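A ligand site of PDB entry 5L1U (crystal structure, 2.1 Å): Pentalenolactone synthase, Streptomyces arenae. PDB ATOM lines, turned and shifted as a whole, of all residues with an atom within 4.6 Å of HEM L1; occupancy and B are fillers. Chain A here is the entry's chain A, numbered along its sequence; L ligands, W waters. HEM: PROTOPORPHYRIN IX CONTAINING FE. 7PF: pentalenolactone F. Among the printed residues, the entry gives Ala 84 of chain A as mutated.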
ATOM      1  N   LEU A  63     -17.958 -29.692 -37.919  1.00  0.00           N
ATOM      2  CA  LEU A  63     -16.584 -29.186 -37.942  1.00  0.00           C
ATOM      3  C   LEU A  63     -15.961 -29.328 -39.327  1.00  0.00           C
ATOM      4  O   LEU A  63     -15.267 -28.408 -39.792  1.00  0.00           O
ATOM      5  CB  LEU A  63     -15.751 -29.914 -36.875  1.00  0.00           C
ATOM      6  CG  LEU A  63     -14.317 -29.436 -36.655  1.00  0.00           C
ATOM      7  CD1 LEU A  63     -14.305 -28.046 -35.990  1.00  0.00           C
ATOM      8  CD2 LEU A  63     -13.504 -30.434 -35.815  1.00  0.00           C
ATOM      9  N   ALA A  84      -9.540 -33.482 -33.747  1.00  0.00           N
ATOM     10  CA  ALA A  84     -10.948 -33.643 -33.423  1.00  0.00           C
ATOM     11  C   ALA A  84     -11.696 -34.472 -34.475  1.00  0.00           C
ATOM     12  O   ALA A  84     -12.925 -34.394 -34.563  1.00  0.00           O
ATOM     13  CB  ALA A  84     -11.598 -32.273 -33.235  1.00  0.00           C
ATOM     14  N   HIS A  96     -15.660 -39.427 -35.615  1.00  0.00           N
ATOM     15  CA  HIS A  96     -15.959 -38.584 -34.472  1.00  0.00           C
ATOM     16  C   HIS A  96     -16.792 -39.335 -33.445  1.00  0.00           C
ATOM     17  O   HIS A  96     -16.560 -39.201 -32.239  1.00  0.00           O
ATOM     18  CB  HIS A  96     -16.645 -37.289 -34.923  1.00  0.00           C
ATOM     19  CG  HIS A  96     -17.156 -36.461 -33.782  1.00  0.00           C
ATOM     20  ND1 HIS A  96     -16.317 -35.777 -32.920  1.00  0.00           N
ATOM     21  CD2 HIS A  96     -18.407 -36.166 -33.387  1.00  0.00           C
ATOM     22  CE1 HIS A  96     -17.039 -35.132 -32.020  1.00  0.00           C
ATOM     23  NE2 HIS A  96     -18.308 -35.348 -32.288  1.00  0.00           N
ATOM     24  N   ARG A 100     -15.546 -39.848 -29.417  1.00  0.00           N
ATOM     25  CA  ARG A 100     -16.291 -39.561 -28.206  1.00  0.00           C
ATOM     26  C   ARG A 100     -16.555 -40.825 -27.401  1.00  0.00           C
ATOM     27  O   ARG A 100     -16.428 -40.812 -26.167  1.00  0.00           O
ATOM     28  CB  ARG A 100     -17.588 -38.832 -28.557  1.00  0.00           C
ATOM     29  CG  ARG A 100     -17.234 -37.482 -29.181  1.00  0.00           C
ATOM     30  CD  ARG A 100     -18.319 -36.462 -29.082  1.00  0.00           C
ATOM     31  NE  ARG A 100     -18.803 -36.186 -27.731  1.00  0.00           N
ATOM     32  CZ  ARG A 100     -18.517 -35.090 -27.021  1.00  0.00           C
ATOM     33  NH1 ARG A 100     -17.687 -34.167 -27.507  1.00  0.00           N
ATOM     34  NH2 ARG A 100     -19.061 -34.914 -25.835  1.00  0.00           N
ATOM     35  N   LEU A 103     -13.268 -41.546 -25.537  1.00  0.00           N
ATOM     36  CA  LEU A 103     -12.765 -40.579 -24.566  1.00  0.00           C
ATOM     37  C   LEU A 103     -13.699 -40.372 -23.376  1.00  0.00           C
ATOM     38  O   LEU A 103     -13.235 -40.191 -22.242  1.00  0.00           O
ATOM     39  CB  LEU A 103     -12.510 -39.226 -25.250  1.00  0.00           C
ATOM     40  CG  LEU A 103     -11.244 -39.162 -26.113  1.00  0.00           C
ATOM     41  CD1 LEU A 103     -11.074 -37.773 -26.733  1.00  0.00           C
ATOM     42  CD2 LEU A 103     -10.022 -39.511 -25.250  1.00  0.00           C
ATOM     43  N   PHE A 107     -13.223 -40.278 -18.323  1.00  0.00           N
ATOM     44  CA  PHE A 107     -13.445 -39.227 -17.338  1.00  0.00           C
ATOM     45  C   PHE A 107     -14.568 -39.669 -16.413  1.00  0.00           C
ATOM     46  O   PHE A 107     -15.556 -38.964 -16.211  1.00  0.00           O
ATOM     47  CB  PHE A 107     -13.750 -37.897 -18.043  1.00  0.00           C
ATOM     48  CG  PHE A 107     -12.588 -37.391 -18.888  1.00  0.00           C
ATOM     49  CD1 PHE A 107     -12.388 -37.852 -20.186  1.00  0.00           C
ATOM     50  CD2 PHE A 107     -11.687 -36.475 -18.374  1.00  0.00           C
ATOM     51  CE1 PHE A 107     -11.327 -37.407 -20.953  1.00  0.00           C
ATOM     52  CE2 PHE A 107     -10.606 -36.026 -19.120  1.00  0.00           C
ATOM     53  CZ  PHE A 107     -10.419 -36.488 -20.418  1.00  0.00           C
ATOM     54  N   LEU A 155      -3.571 -37.659 -15.851  1.00  0.00           N
ATOM     55  CA  LEU A 155      -4.373 -38.371 -16.848  1.00  0.00           C
ATOM     56  C   LEU A 155      -3.526 -39.319 -17.673  1.00  0.00           C
ATOM     57  O   LEU A 155      -3.950 -40.439 -17.971  1.00  0.00           O
ATOM     58  CB  LEU A 155      -5.075 -37.379 -17.785  1.00  0.00           C
ATOM     59  CG  LEU A 155      -6.158 -36.476 -17.199  1.00  0.00           C
ATOM     60  CD1 LEU A 155      -6.575 -35.451 -18.256  1.00  0.00           C
ATOM     61  CD2 LEU A 155      -7.353 -37.333 -16.763  1.00  0.00           C
ATOM     62  N   VAL A 232      -5.977 -35.242 -25.882  1.00  0.00           N
ATOM     63  CA  VAL A 232      -6.020 -34.972 -24.444  1.00  0.00           C
ATOM     64  C   VAL A 232      -4.881 -34.036 -24.053  1.00  0.00           C
ATOM     65  O   VAL A 232      -5.076 -33.090 -23.278  1.00  0.00           O
ATOM     66  CB  VAL A 232      -5.961 -36.291 -23.649  1.00  0.00           C
ATOM     67  CG1 VAL A 232      -5.686 -36.009 -22.170  1.00  0.00           C
ATOM     68  CG2 VAL A 232      -7.271 -37.070 -23.803  1.00  0.00           C
ATOM     69  N   PHE A 235      -5.613 -30.413 -26.073  1.00  0.00           N
ATOM     70  CA  PHE A 235      -6.846 -29.731 -25.666  1.00  0.00           C
ATOM     71  C   PHE A 235      -6.986 -29.658 -24.140  1.00  0.00           C
ATOM     72  O   PHE A 235      -7.865 -28.930 -23.640  1.00  0.00           O
ATOM     73  CB  PHE A 235      -8.087 -30.457 -26.233  1.00  0.00           C
ATOM     74  CG  PHE A 235      -8.131 -30.542 -27.761  1.00  0.00           C
ATOM     75  CD1 PHE A 235      -7.315 -29.717 -28.547  1.00  0.00           C
ATOM     76  CD2 PHE A 235      -9.001 -31.410 -28.396  1.00  0.00           C
ATOM     77  CE1 PHE A 235      -7.359 -29.777 -29.932  1.00  0.00           C
ATOM     78  CE2 PHE A 235      -9.049 -31.491 -29.787  1.00  0.00           C
ATOM     79  CZ  PHE A 235      -8.233 -30.669 -30.563  1.00  0.00           C
ATOM     80  N   GLY A 236      -6.183 -30.414 -23.394  1.00  0.00           N
ATOM     81  CA  GLY A 236      -6.456 -30.695 -21.993  1.00  0.00           C
ATOM     82  C   GLY A 236      -5.750 -29.872 -20.941  1.00  0.00           C
ATOM     83  O   GLY A 236      -5.989 -30.093 -19.752  1.00  0.00           O
ATOM     84  N   THR A 239      -6.196 -24.387 -22.418  1.00  0.00           N
ATOM     85  CA  THR A 239      -7.398 -23.571 -22.244  1.00  0.00           C
ATOM     86  C   THR A 239      -7.756 -23.403 -20.770  1.00  0.00           C
ATOM     87  O   THR A 239      -8.276 -22.352 -20.376  1.00  0.00           O
ATOM     88  CB  THR A 239      -8.583 -24.192 -23.010  1.00  0.00           C
ATOM     89  OG1 THR A 239      -8.797 -25.535 -22.563  1.00  0.00           O
ATOM     90  CG2 THR A 239      -8.323 -24.204 -24.530  1.00  0.00           C
ATOM     91  N   THR A 240      -7.504 -24.427 -19.941  1.00  0.00           N
ATOM     92  CA  THR A 240      -7.707 -24.293 -18.500  1.00  0.00           C
ATOM     93  C   THR A 240      -6.734 -23.288 -17.899  1.00  0.00           C
ATOM     94  O   THR A 240      -7.126 -22.489 -17.029  1.00  0.00           O
ATOM     95  CB  THR A 240      -7.540 -25.651 -17.822  1.00  0.00           C
ATOM     96  OG1 THR A 240      -8.322 -26.618 -18.529  1.00  0.00           O
ATOM     97  CG2 THR A 240      -7.995 -25.608 -16.374  1.00  0.00           C
ATOM     98  N   ARG A 243      -8.153 -19.957 -18.484  1.00  0.00           N
ATOM     99  CA  ARG A 243      -9.303 -19.606 -17.655  1.00  0.00           C
ATOM    100  C   ARG A 243      -8.906 -19.261 -16.231  1.00  0.00           C
ATOM    101  O   ARG A 243      -9.586 -18.444 -15.582  1.00  0.00           O
ATOM    102  CB  ARG A 243     -10.332 -20.740 -17.658  1.00  0.00           C
ATOM    103  CG  ARG A 243     -11.025 -20.975 -19.024  1.00  0.00           C
ATOM    104  CD  ARG A 243     -11.153 -19.671 -19.802  1.00  0.00           C
ATOM    105  NE  ARG A 243     -11.794 -19.819 -21.112  1.00  0.00           N
ATOM    106  CZ  ARG A 243     -11.167 -20.201 -22.215  1.00  0.00           C
ATOM    107  NH1 ARG A 243      -9.869 -20.517 -22.168  1.00  0.00           N
ATOM    108  NH2 ARG A 243     -11.819 -20.254 -23.371  1.00  0.00           N
ATOM    109  N   LEU A 276     -16.238 -18.594 -16.476  1.00  0.00           N
ATOM    110  CA  LEU A 276     -16.313 -19.224 -17.790  1.00  0.00           C
ATOM    111  C   LEU A 276     -17.187 -18.432 -18.743  1.00  0.00           C
ATOM    112  O   LEU A 276     -16.871 -18.295 -19.938  1.00  0.00           O
ATOM    113  CB  LEU A 276     -16.857 -20.649 -17.656  1.00  0.00           C
ATOM    114  CG  LEU A 276     -16.051 -21.652 -16.828  1.00  0.00           C
ATOM    115  CD1 LEU A 276     -16.841 -22.921 -16.560  1.00  0.00           C
ATOM    116  CD2 LEU A 276     -14.790 -21.989 -17.601  1.00  0.00           C
ATOM    117  N   ILE A 289     -16.616 -20.789 -32.260  1.00  0.00           N
ATOM    118  CA  ILE A 289     -16.590 -22.190 -32.669  1.00  0.00           C
ATOM    119  C   ILE A 289     -16.840 -22.237 -34.172  1.00  0.00           C
ATOM    120  O   ILE A 289     -17.932 -21.839 -34.614  1.00  0.00           O
ATOM    121  CB  ILE A 289     -17.617 -23.036 -31.917  1.00  0.00           C
ATOM    122  CG1 ILE A 289     -17.277 -23.122 -30.423  1.00  0.00           C
ATOM    123  CG2 ILE A 289     -17.694 -24.423 -32.550  1.00  0.00           C
ATOM    124  CD1 ILE A 289     -18.287 -23.942 -29.623  1.00  0.00           C
ATOM    125  N   ARG A 291     -17.621 -23.766 -37.949  1.00  0.00           N
ATOM    126  CA  ARG A 291     -18.421 -24.840 -38.510  1.00  0.00           C
ATOM    127  C   ARG A 291     -18.595 -24.608 -40.015  1.00  0.00           C
ATOM    128  O   ARG A 291     -18.382 -23.507 -40.524  1.00  0.00           O
ATOM    129  CB  ARG A 291     -19.795 -24.908 -37.836  1.00  0.00           C
ATOM    130  CG  ARG A 291     -19.803 -25.315 -36.360  1.00  0.00           C
ATOM    131  CD  ARG A 291     -19.449 -26.791 -36.189  1.00  0.00           C
ATOM    132  NE  ARG A 291     -19.618 -27.252 -34.812  1.00  0.00           N
ATOM    133  CZ  ARG A 291     -18.641 -27.425 -33.936  1.00  0.00           C
ATOM    134  NH1 ARG A 291     -17.385 -27.137 -34.283  1.00  0.00           N
ATOM    135  NH2 ARG A 291     -18.914 -27.877 -32.711  1.00  0.00           N
ATOM    136  N   ILE A 314     -19.586 -18.059 -29.165  1.00  0.00           N
ATOM    137  CA  ILE A 314     -19.992 -18.456 -27.818  1.00  0.00           C
ATOM    138  C   ILE A 314     -19.656 -17.368 -26.808  1.00  0.00           C
ATOM    139  O   ILE A 314     -20.380 -17.190 -25.817  1.00  0.00           O
ATOM    140  CB  ILE A 314     -19.331 -19.810 -27.458  1.00  0.00           C
ATOM    141  CG1 ILE A 314     -17.798 -19.721 -27.554  1.00  0.00           C
ATOM    142  CG2 ILE A 314     -19.873 -20.929 -28.338  1.00  0.00           C
ATOM    143  CD1 ILE A 314     -17.073 -20.998 -27.046  1.00  0.00           C
ATOM    144  N   ALA A 342     -19.509 -21.720 -22.849  1.00  0.00           N
ATOM    145  CA  ALA A 342     -18.038 -21.706 -22.925  1.00  0.00           C
ATOM    146  C   ALA A 342     -17.434 -23.088 -23.168  1.00  0.00           C
ATOM    147  O   ALA A 342     -16.261 -23.169 -23.593  1.00  0.00           O
ATOM    148  CB  ALA A 342     -17.432 -21.133 -21.634  1.00  0.00           C
ATOM    149  N   PHE A 343     -18.144 -24.166 -22.876  1.00  0.00           N
ATOM    150  CA  PHE A 343     -17.714 -25.508 -23.240  1.00  0.00           C
ATOM    151  C   PHE A 343     -18.395 -25.999 -24.516  1.00  0.00           C
ATOM    152  O   PHE A 343     -18.308 -27.186 -24.840  1.00  0.00           O
ATOM    153  CB  PHE A 343     -18.018 -26.498 -22.102  1.00  0.00           C
ATOM    154  CG  PHE A 343     -17.199 -26.275 -20.856  1.00  0.00           C
ATOM    155  CD1 PHE A 343     -15.819 -26.335 -20.880  1.00  0.00           C
ATOM    156  CD2 PHE A 343     -17.834 -26.016 -19.622  1.00  0.00           C
ATOM    157  CE1 PHE A 343     -15.065 -26.143 -19.715  1.00  0.00           C
ATOM    158  CE2 PHE A 343     -17.086 -25.834 -18.450  1.00  0.00           C
ATOM    159  CZ  PHE A 343     -15.707 -25.888 -18.493  1.00  0.00           C
ATOM    160  N   GLY A 344     -19.090 -25.105 -25.222  1.00  0.00           N
ATOM    161  CA  GLY A 344     -19.853 -25.544 -26.367  1.00  0.00           C
ATOM    162  C   GLY A 344     -21.146 -26.248 -25.966  1.00  0.00           C
ATOM    163  O   GLY A 344     -21.673 -26.077 -24.855  1.00  0.00           O
ATOM    164  N   ALA A 347     -23.054 -31.998 -30.259  1.00  0.00           N
ATOM    165  CA  ALA A 347     -22.247 -33.170 -30.609  1.00  0.00           C
ATOM    166  C   ALA A 347     -20.798 -33.060 -30.145  1.00  0.00           C
ATOM    167  O   ALA A 347     -20.166 -34.085 -29.853  1.00  0.00           O
ATOM    168  CB  ALA A 347     -22.293 -33.399 -32.127  1.00  0.00           C
ATOM    169  N   ARG A 348     -20.245 -31.849 -30.061  1.00  0.00           N
ATOM    170  CA  ARG A 348     -18.843 -31.682 -29.715  1.00  0.00           C
ATOM    171  C   ARG A 348     -18.637 -31.028 -28.343  1.00  0.00           C
ATOM    172  O   ARG A 348     -17.531 -30.562 -28.040  1.00  0.00           O
ATOM    173  CB  ARG A 348     -18.134 -30.891 -30.813  1.00  0.00           C
ATOM    174  CG  ARG A 348     -17.756 -31.777 -32.021  1.00  0.00           C
ATOM    175  CD  ARG A 348     -17.307 -30.994 -33.244  1.00  0.00           C
ATOM    176  NE  ARG A 348     -17.013 -31.858 -34.392  1.00  0.00           N
ATOM    177  CZ  ARG A 348     -15.961 -32.686 -34.475  1.00  0.00           C
ATOM    178  NH1 ARG A 348     -15.087 -32.759 -33.485  1.00  0.00           N
ATOM    179  NH2 ARG A 348     -15.770 -33.437 -35.557  1.00  0.00           N
ATOM    180  N   HIS A 349     -19.681 -30.982 -27.513  1.00  0.00           N
ATOM    181  CA  HIS A 349     -19.609 -30.500 -26.128  1.00  0.00           C
ATOM    182  C   HIS A 349     -18.352 -31.011 -25.429  1.00  0.00           C
ATOM    183  O   HIS A 349     -18.087 -32.217 -25.406  1.00  0.00           O
ATOM    184  CB  HIS A 349     -20.857 -30.975 -25.378  1.00  0.00           C
ATOM    185  CG  HIS A 349     -21.206 -30.146 -24.186  1.00  0.00           C
ATOM    186  ND1 HIS A 349     -22.312 -30.418 -23.398  1.00  0.00           N
ATOM    187  CD2 HIS A 349     -20.629 -29.047 -23.646  1.00  0.00           C
ATOM    188  CE1 HIS A 349     -22.383 -29.535 -22.424  1.00  0.00           C
ATOM    189  NE2 HIS A 349     -21.375 -28.684 -22.558  1.00  0.00           N
ATOM    190  N   CYS A 350     -17.567 -30.081 -24.869  1.00  0.00           N
ATOM    191  CA  CYS A 350     -16.245 -30.365 -24.322  1.00  0.00           C
ATOM    192  C   CYS A 350     -16.226 -31.622 -23.456  1.00  0.00           C
ATOM    193  O   CYS A 350     -17.037 -31.786 -22.535  1.00  0.00           O
ATOM    194  CB  CYS A 350     -15.783 -29.172 -23.481  1.00  0.00           C
ATOM    195  SG  CYS A 350     -14.427 -29.517 -22.317  1.00  0.00           S
ATOM    196  N   ILE A 351     -15.301 -32.522 -23.757  1.00  0.00           N
ATOM    197  CA  ILE A 351     -15.226 -33.792 -23.041  1.00  0.00           C
ATOM    198  C   ILE A 351     -14.647 -33.622 -21.640  1.00  0.00           C
ATOM    199  O   ILE A 351     -15.040 -34.338 -20.712  1.00  0.00           O
ATOM    200  CB  ILE A 351     -14.434 -34.807 -23.896  1.00  0.00           C
ATOM    201  CG1 ILE A 351     -15.313 -35.335 -25.046  1.00  0.00           C
ATOM    202  CG2 ILE A 351     -13.933 -35.976 -23.062  1.00  0.00           C
ATOM    203  CD1 ILE A 351     -14.573 -36.145 -26.058  1.00  0.00           C
ATOM    204  N   GLY A 352     -13.743 -32.660 -21.427  1.00  0.00           N
ATOM    205  CA  GLY A 352     -13.149 -32.475 -20.116  1.00  0.00           C
ATOM    206  C   GLY A 352     -13.841 -31.481 -19.195  1.00  0.00           C
ATOM    207  O   GLY A 352     -13.253 -31.089 -18.177  1.00  0.00           O
ATOM    208  N   LEU A 355     -13.995 -32.131 -15.442  1.00  0.00           N
ATOM    209  CA  LEU A 355     -12.668 -32.039 -14.856  1.00  0.00           C
ATOM    210  C   LEU A 355     -12.161 -30.594 -14.828  1.00  0.00           C
ATOM    211  O   LEU A 355     -11.557 -30.152 -13.847  1.00  0.00           O
ATOM    212  CB  LEU A 355     -11.699 -32.954 -15.632  1.00  0.00           C
ATOM    213  CG  LEU A 355     -10.228 -32.885 -15.222  1.00  0.00           C
ATOM    214  CD1 LEU A 355     -10.067 -33.280 -13.755  1.00  0.00           C
ATOM    215  CD2 LEU A 355      -9.352 -33.772 -16.113  1.00  0.00           C
ATOM    216  N   ALA A 356     -12.420 -29.832 -15.902  1.00  0.00           N
ATOM    217  CA  ALA A 356     -12.035 -28.423 -15.913  1.00  0.00           C
ATOM    218  C   ALA A 356     -12.723 -27.644 -14.796  1.00  0.00           C
ATOM    219  O   ALA A 356     -12.104 -26.776 -14.158  1.00  0.00           O
ATOM    220  CB  ALA A 356     -12.345 -27.798 -17.278  1.00  0.00           C
ATOM    221  N   GLU A 359     -10.987 -28.347 -11.488  1.00  0.00           N
ATOM    222  CA  GLU A 359      -9.748 -27.573 -11.355  1.00  0.00           C
ATOM    223  C   GLU A 359     -10.028 -26.127 -10.993  1.00  0.00           C
ATOM    224  O   GLU A 359      -9.465 -25.597 -10.028  1.00  0.00           O
ATOM    225  CB  GLU A 359      -8.954 -27.620 -12.673  1.00  0.00           C
ATOM    226  CG  GLU A 359      -8.392 -28.987 -13.036  1.00  0.00           C
ATOM    227  CD  GLU A 359      -7.510 -28.907 -14.265  1.00  0.00           C
ATOM    228  OE1 GLU A 359      -6.566 -28.084 -14.261  1.00  0.00           O
ATOM    229  OE2 GLU A 359      -7.752 -29.646 -15.245  1.00  0.00           O
ATOM    230  N   LEU A 360     -10.904 -25.466 -11.756  1.00  0.00           N
ATOM    231  CA  LEU A 360     -11.169 -24.054 -11.498  1.00  0.00           C
ATOM    232  C   LEU A 360     -11.815 -23.850 -10.135  1.00  0.00           C
ATOM    233  O   LEU A 360     -11.497 -22.884  -9.423  1.00  0.00           O
ATOM    234  CB  LEU A 360     -12.053 -23.470 -12.607  1.00  0.00           C
ATOM    235  CG  LEU A 360     -11.440 -23.431 -14.002  1.00  0.00           C
ATOM    236  CD1 LEU A 360     -12.506 -22.994 -15.006  1.00  0.00           C
ATOM    237  CD2 LEU A 360     -10.203 -22.492 -14.070  1.00  0.00           C
HETATM  238  CHA HEM L   1     -13.996 -29.503 -26.920  1.00  0.00           C
HETATM  239  CHB HEM L   1     -13.639 -25.501 -24.185  1.00  0.00           C
HETATM  240  CHC HEM L   1     -10.927 -27.930 -20.988  1.00  0.00           C
HETATM  241  CHD HEM L   1     -11.020 -31.855 -23.849  1.00  0.00           C
HETATM  242  C1A HEM L   1     -14.205 -28.240 -26.436  1.00  0.00           C
HETATM  243  C2A HEM L   1     -15.070 -27.222 -27.020  1.00  0.00           C
HETATM  244  C3A HEM L   1     -14.966 -26.115 -26.262  1.00  0.00           C
HETATM  245  C4A HEM L   1     -14.038 -26.391 -25.166  1.00  0.00           C
HETATM  246  CMA HEM L   1     -15.693 -24.773 -26.489  1.00  0.00           C
HETATM  247  CAA HEM L   1     -15.971 -27.418 -28.268  1.00  0.00           C
HETATM  248  CBA HEM L   1     -15.217 -27.276 -29.591  1.00  0.00           C
HETATM  249  CGA HEM L   1     -16.149 -27.466 -30.774  1.00  0.00           C
HETATM  250  O1A HEM L   1     -17.395 -27.430 -30.581  1.00  0.00           O
HETATM  251  O2A HEM L   1     -15.641 -27.652 -31.921  1.00  0.00           O
HETATM  252  C1B HEM L   1     -12.881 -25.790 -23.080  1.00  0.00           C
HETATM  253  C2B HEM L   1     -12.579 -24.900 -21.973  1.00  0.00           C
HETATM  254  C3B HEM L   1     -11.810 -25.587 -21.102  1.00  0.00           C
HETATM  255  C4B HEM L   1     -11.631 -26.933 -21.621  1.00  0.00           C
HETATM  256  CMB HEM L   1     -13.062 -23.428 -21.872  1.00  0.00           C
HETATM  257  CAB HEM L   1     -11.216 -25.154 -19.748  1.00  0.00           C
HETATM  258  CBB HEM L   1     -11.854 -24.316 -18.926  1.00  0.00           C
HETATM  259  C1C HEM L   1     -10.744 -29.219 -21.448  1.00  0.00           C
HETATM  260  C2C HEM L   1     -10.055 -30.278 -20.739  1.00  0.00           C
HETATM  261  C3C HEM L   1     -10.082 -31.370 -21.535  1.00  0.00           C
HETATM  262  C4C HEM L   1     -10.779 -31.026 -22.770  1.00  0.00           C
HETATM  263  CMC HEM L   1      -9.464 -30.098 -19.315  1.00  0.00           C
HETATM  264  CAC HEM L   1      -9.503 -32.784 -21.285  1.00  0.00           C
HETATM  265  CBC HEM L   1      -8.568 -33.081 -20.363  1.00  0.00           C
HETATM  266  C1D HEM L   1     -11.774 -31.542 -24.958  1.00  0.00           C
HETATM  267  C2D HEM L   1     -11.936 -32.347 -26.156  1.00  0.00           C
HETATM  268  C3D HEM L   1     -12.742 -31.702 -27.008  1.00  0.00           C
HETATM  269  C4D HEM L   1     -13.131 -30.453 -26.390  1.00  0.00           C
HETATM  270  CMD HEM L   1     -11.262 -33.719 -26.397  1.00  0.00           C
HETATM  271  CAD HEM L   1     -13.177 -32.196 -28.403  1.00  0.00           C
HETATM  272  CBD HEM L   1     -14.684 -32.501 -28.392  1.00  0.00           C
HETATM  273  CGD HEM L   1     -15.159 -32.922 -29.754  1.00  0.00           C
HETATM  274  O1D HEM L   1     -16.041 -33.818 -29.802  1.00  0.00           O
HETATM  275  O2D HEM L   1     -14.661 -32.375 -30.786  1.00  0.00           O
HETATM  276  NA  HEM L   1     -13.597 -27.699 -25.312  1.00  0.00           N
HETATM  277  NB  HEM L   1     -12.278 -27.015 -22.827  1.00  0.00           N
HETATM  278  NC  HEM L   1     -11.163 -29.712 -22.665  1.00  0.00           N
HETATM  279  ND  HEM L   1     -12.532 -30.396 -25.149  1.00  0.00           N
HETATM  280 FE   HEM L   1     -12.601 -28.815 -23.841  1.00  0.00          FE
HETATM  281  C1  7PF L   2     -11.721 -26.226 -27.566  1.00  0.00           C
HETATM  282  C2  7PF L   2     -10.631 -26.618 -28.584  1.00  0.00           C
HETATM  283  C15 7PF L   2     -10.862 -28.070 -29.025  1.00  0.00           C
HETATM  284  C14 7PF L   2      -9.223 -26.494 -27.969  1.00  0.00           C
HETATM  285  C7  7PF L   2     -11.835 -23.758 -26.953  1.00  0.00           C
HETATM  286  C12 7PF L   2     -10.186 -22.221 -29.530  1.00  0.00           C
HETATM  287  C10 7PF L   2     -13.546 -22.822 -29.732  1.00  0.00           C
HETATM  288  C3  7PF L   2     -10.890 -25.680 -29.772  1.00  0.00           C
HETATM  289  C13 7PF L   2     -10.253 -21.983 -26.609  1.00  0.00           C
HETATM  290  C11 7PF L   2     -11.582 -23.180 -31.261  1.00  0.00           C
HETATM  291  C6  7PF L   2     -10.753 -23.024 -27.331  1.00  0.00           C
HETATM  292  C8  7PF L   2     -12.182 -24.774 -27.910  1.00  0.00           C
HETATM  293  C5  7PF L   2     -10.272 -23.457 -28.583  1.00  0.00           C
HETATM  294  C9  7PF L   2     -12.311 -23.616 -30.161  1.00  0.00           C
HETATM  295  C4  7PF L   2     -11.397 -24.353 -29.151  1.00  0.00           C
HETATM  296  O4  7PF L   2     -10.811 -21.571 -25.571  1.00  0.00           O
HETATM  297  O2  7PF L   2     -11.970 -23.443 -32.410  1.00  0.00           O
HETATM  298  O5  7PF L   2      -9.189 -21.397 -26.927  1.00  0.00           O
HETATM  299  O3  7PF L   2     -10.409 -22.530 -30.966  1.00  0.00           O
HETATM  300  O1  7PF L   2     -13.640 -24.136 -30.394  1.00  0.00           O
HETATM  301  O   HOH W   1      -7.579 -27.282 -21.095  1.00  0.00           O
HETATM  302  O   HOH W   2     -13.667 -29.712 -31.872  1.00  0.00           O
HETATM  303  O   HOH W   3      -9.734 -27.197 -24.509  1.00  0.00           O
HETATM  304  O   HOH W   4     -19.426 -27.802 -28.967  1.00  0.00           O
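The side-chain sulfur (SG) of Cys 350 sits close to the backbone NH (N) of Gly 352, 3.3 Å away.
The backbone NH (N) of Cys 350 lies within hydrogen-bond range of the backbone carbonyl oxygen (O) of Phe 343 (3.0 Å).
A ring nitrogen (ND1) of His 96 lies within hydrogen-bond range of the guanidinium group (NH1) of Arg 348 (3.3 Å).
A ring nitrogen (NE2) of His 96 is in hydrogen-bond range of the backbone carbonyl oxygen (O) of Ala 347 (3.3 Å).
The guanidinium group (NE) of Arg 100 sits close to the backbone carbonyl oxygen (O) of Ala 347, 3.3 Å away.
NH1 of Arg 100 lies within hydrogen-bond range of O of His 349, at 2.9 Å.
The backbone carbonyl oxygen of Thr 239 sits at hydrogen-bond distance from the guanidinium group of Arg 243 (3.0 Å).
A ring nitrogen (NE2) of His 349 lies close to the backbone carbonyl oxygen of Gly 344 (3.5 Å).
Water W4 lies within hydrogen-bond range of an oxygen (O1A) of HEM L1 (2.6 Å) and the backbone carbonyl oxygen (O) of Arg 348 (3.5 Å).
Water W3 lies within hydrogen-bond range of the backbone carbonyl oxygen (O) of Phe 235 (2.7 Å) and the side-chain hydroxyl (OG1) of Thr 239 (2.7 Å).
Water W1 lies within hydrogen-bond range of OG1 of Thr 239 (2.6 Å), OG1 of Thr 240 (2.8 Å), O of Phe 235 (3.0 Å) and O of Gly 236 (3.5 Å).
Merely in contact with HEM L1: Ala 84, His 96, Phe 107, Leu 155, Phe 235, Gly 236, Thr 239, Thr 240, Arg 243, Leu 276, Ile 289, Ala 342, Phe 343, Gly 344, Ile 351, Gly 352 and Ala 356.
Hydrophobic or aromatic side chains within 4 Å of HEM L1: Ala 84, His 96, Phe 107, Leu 155, Phe 235, Leu 276, Ile 289, Phe 343 and Ala 356.
Within 4 Å of HEM L1: Ala 84, His 96, Arg 100, Phe 107, Leu 155, Phe 235, Gly 236, Thr 239, Thr 240, Arg 243, Leu 276, Ile 289, Arg 291, Ala 342, Phe 343, Gly 344, Arg 348, Cys 350, Ile 351, Gly 352 and Ala 356.
The nearest printed residue that does not touch HEM L1 is Ile 314 (4.1 Å).
The side-chain sulfur (SG) of Cys 350 binds an iron atom (FE) of HEM L1, at 2.5 Å.
An oxygen (O1A) of HEM L1 is in salt-bridge range of the guanidinium group of Arg 291, 2.7 Å away.
The guanidinium group (NH1) of Arg 348 is in salt-bridge range of an oxygen (O2D) of HEM L1 (2.8 Å).
An oxygen (O1D) of HEM L1 is in salt-bridge range of the guanidinium group of Arg 100 (2.8 Å).
O4 of 7PF L2 lies within salt-bridge range of NH2 of Arg 243 (2.8 Å).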
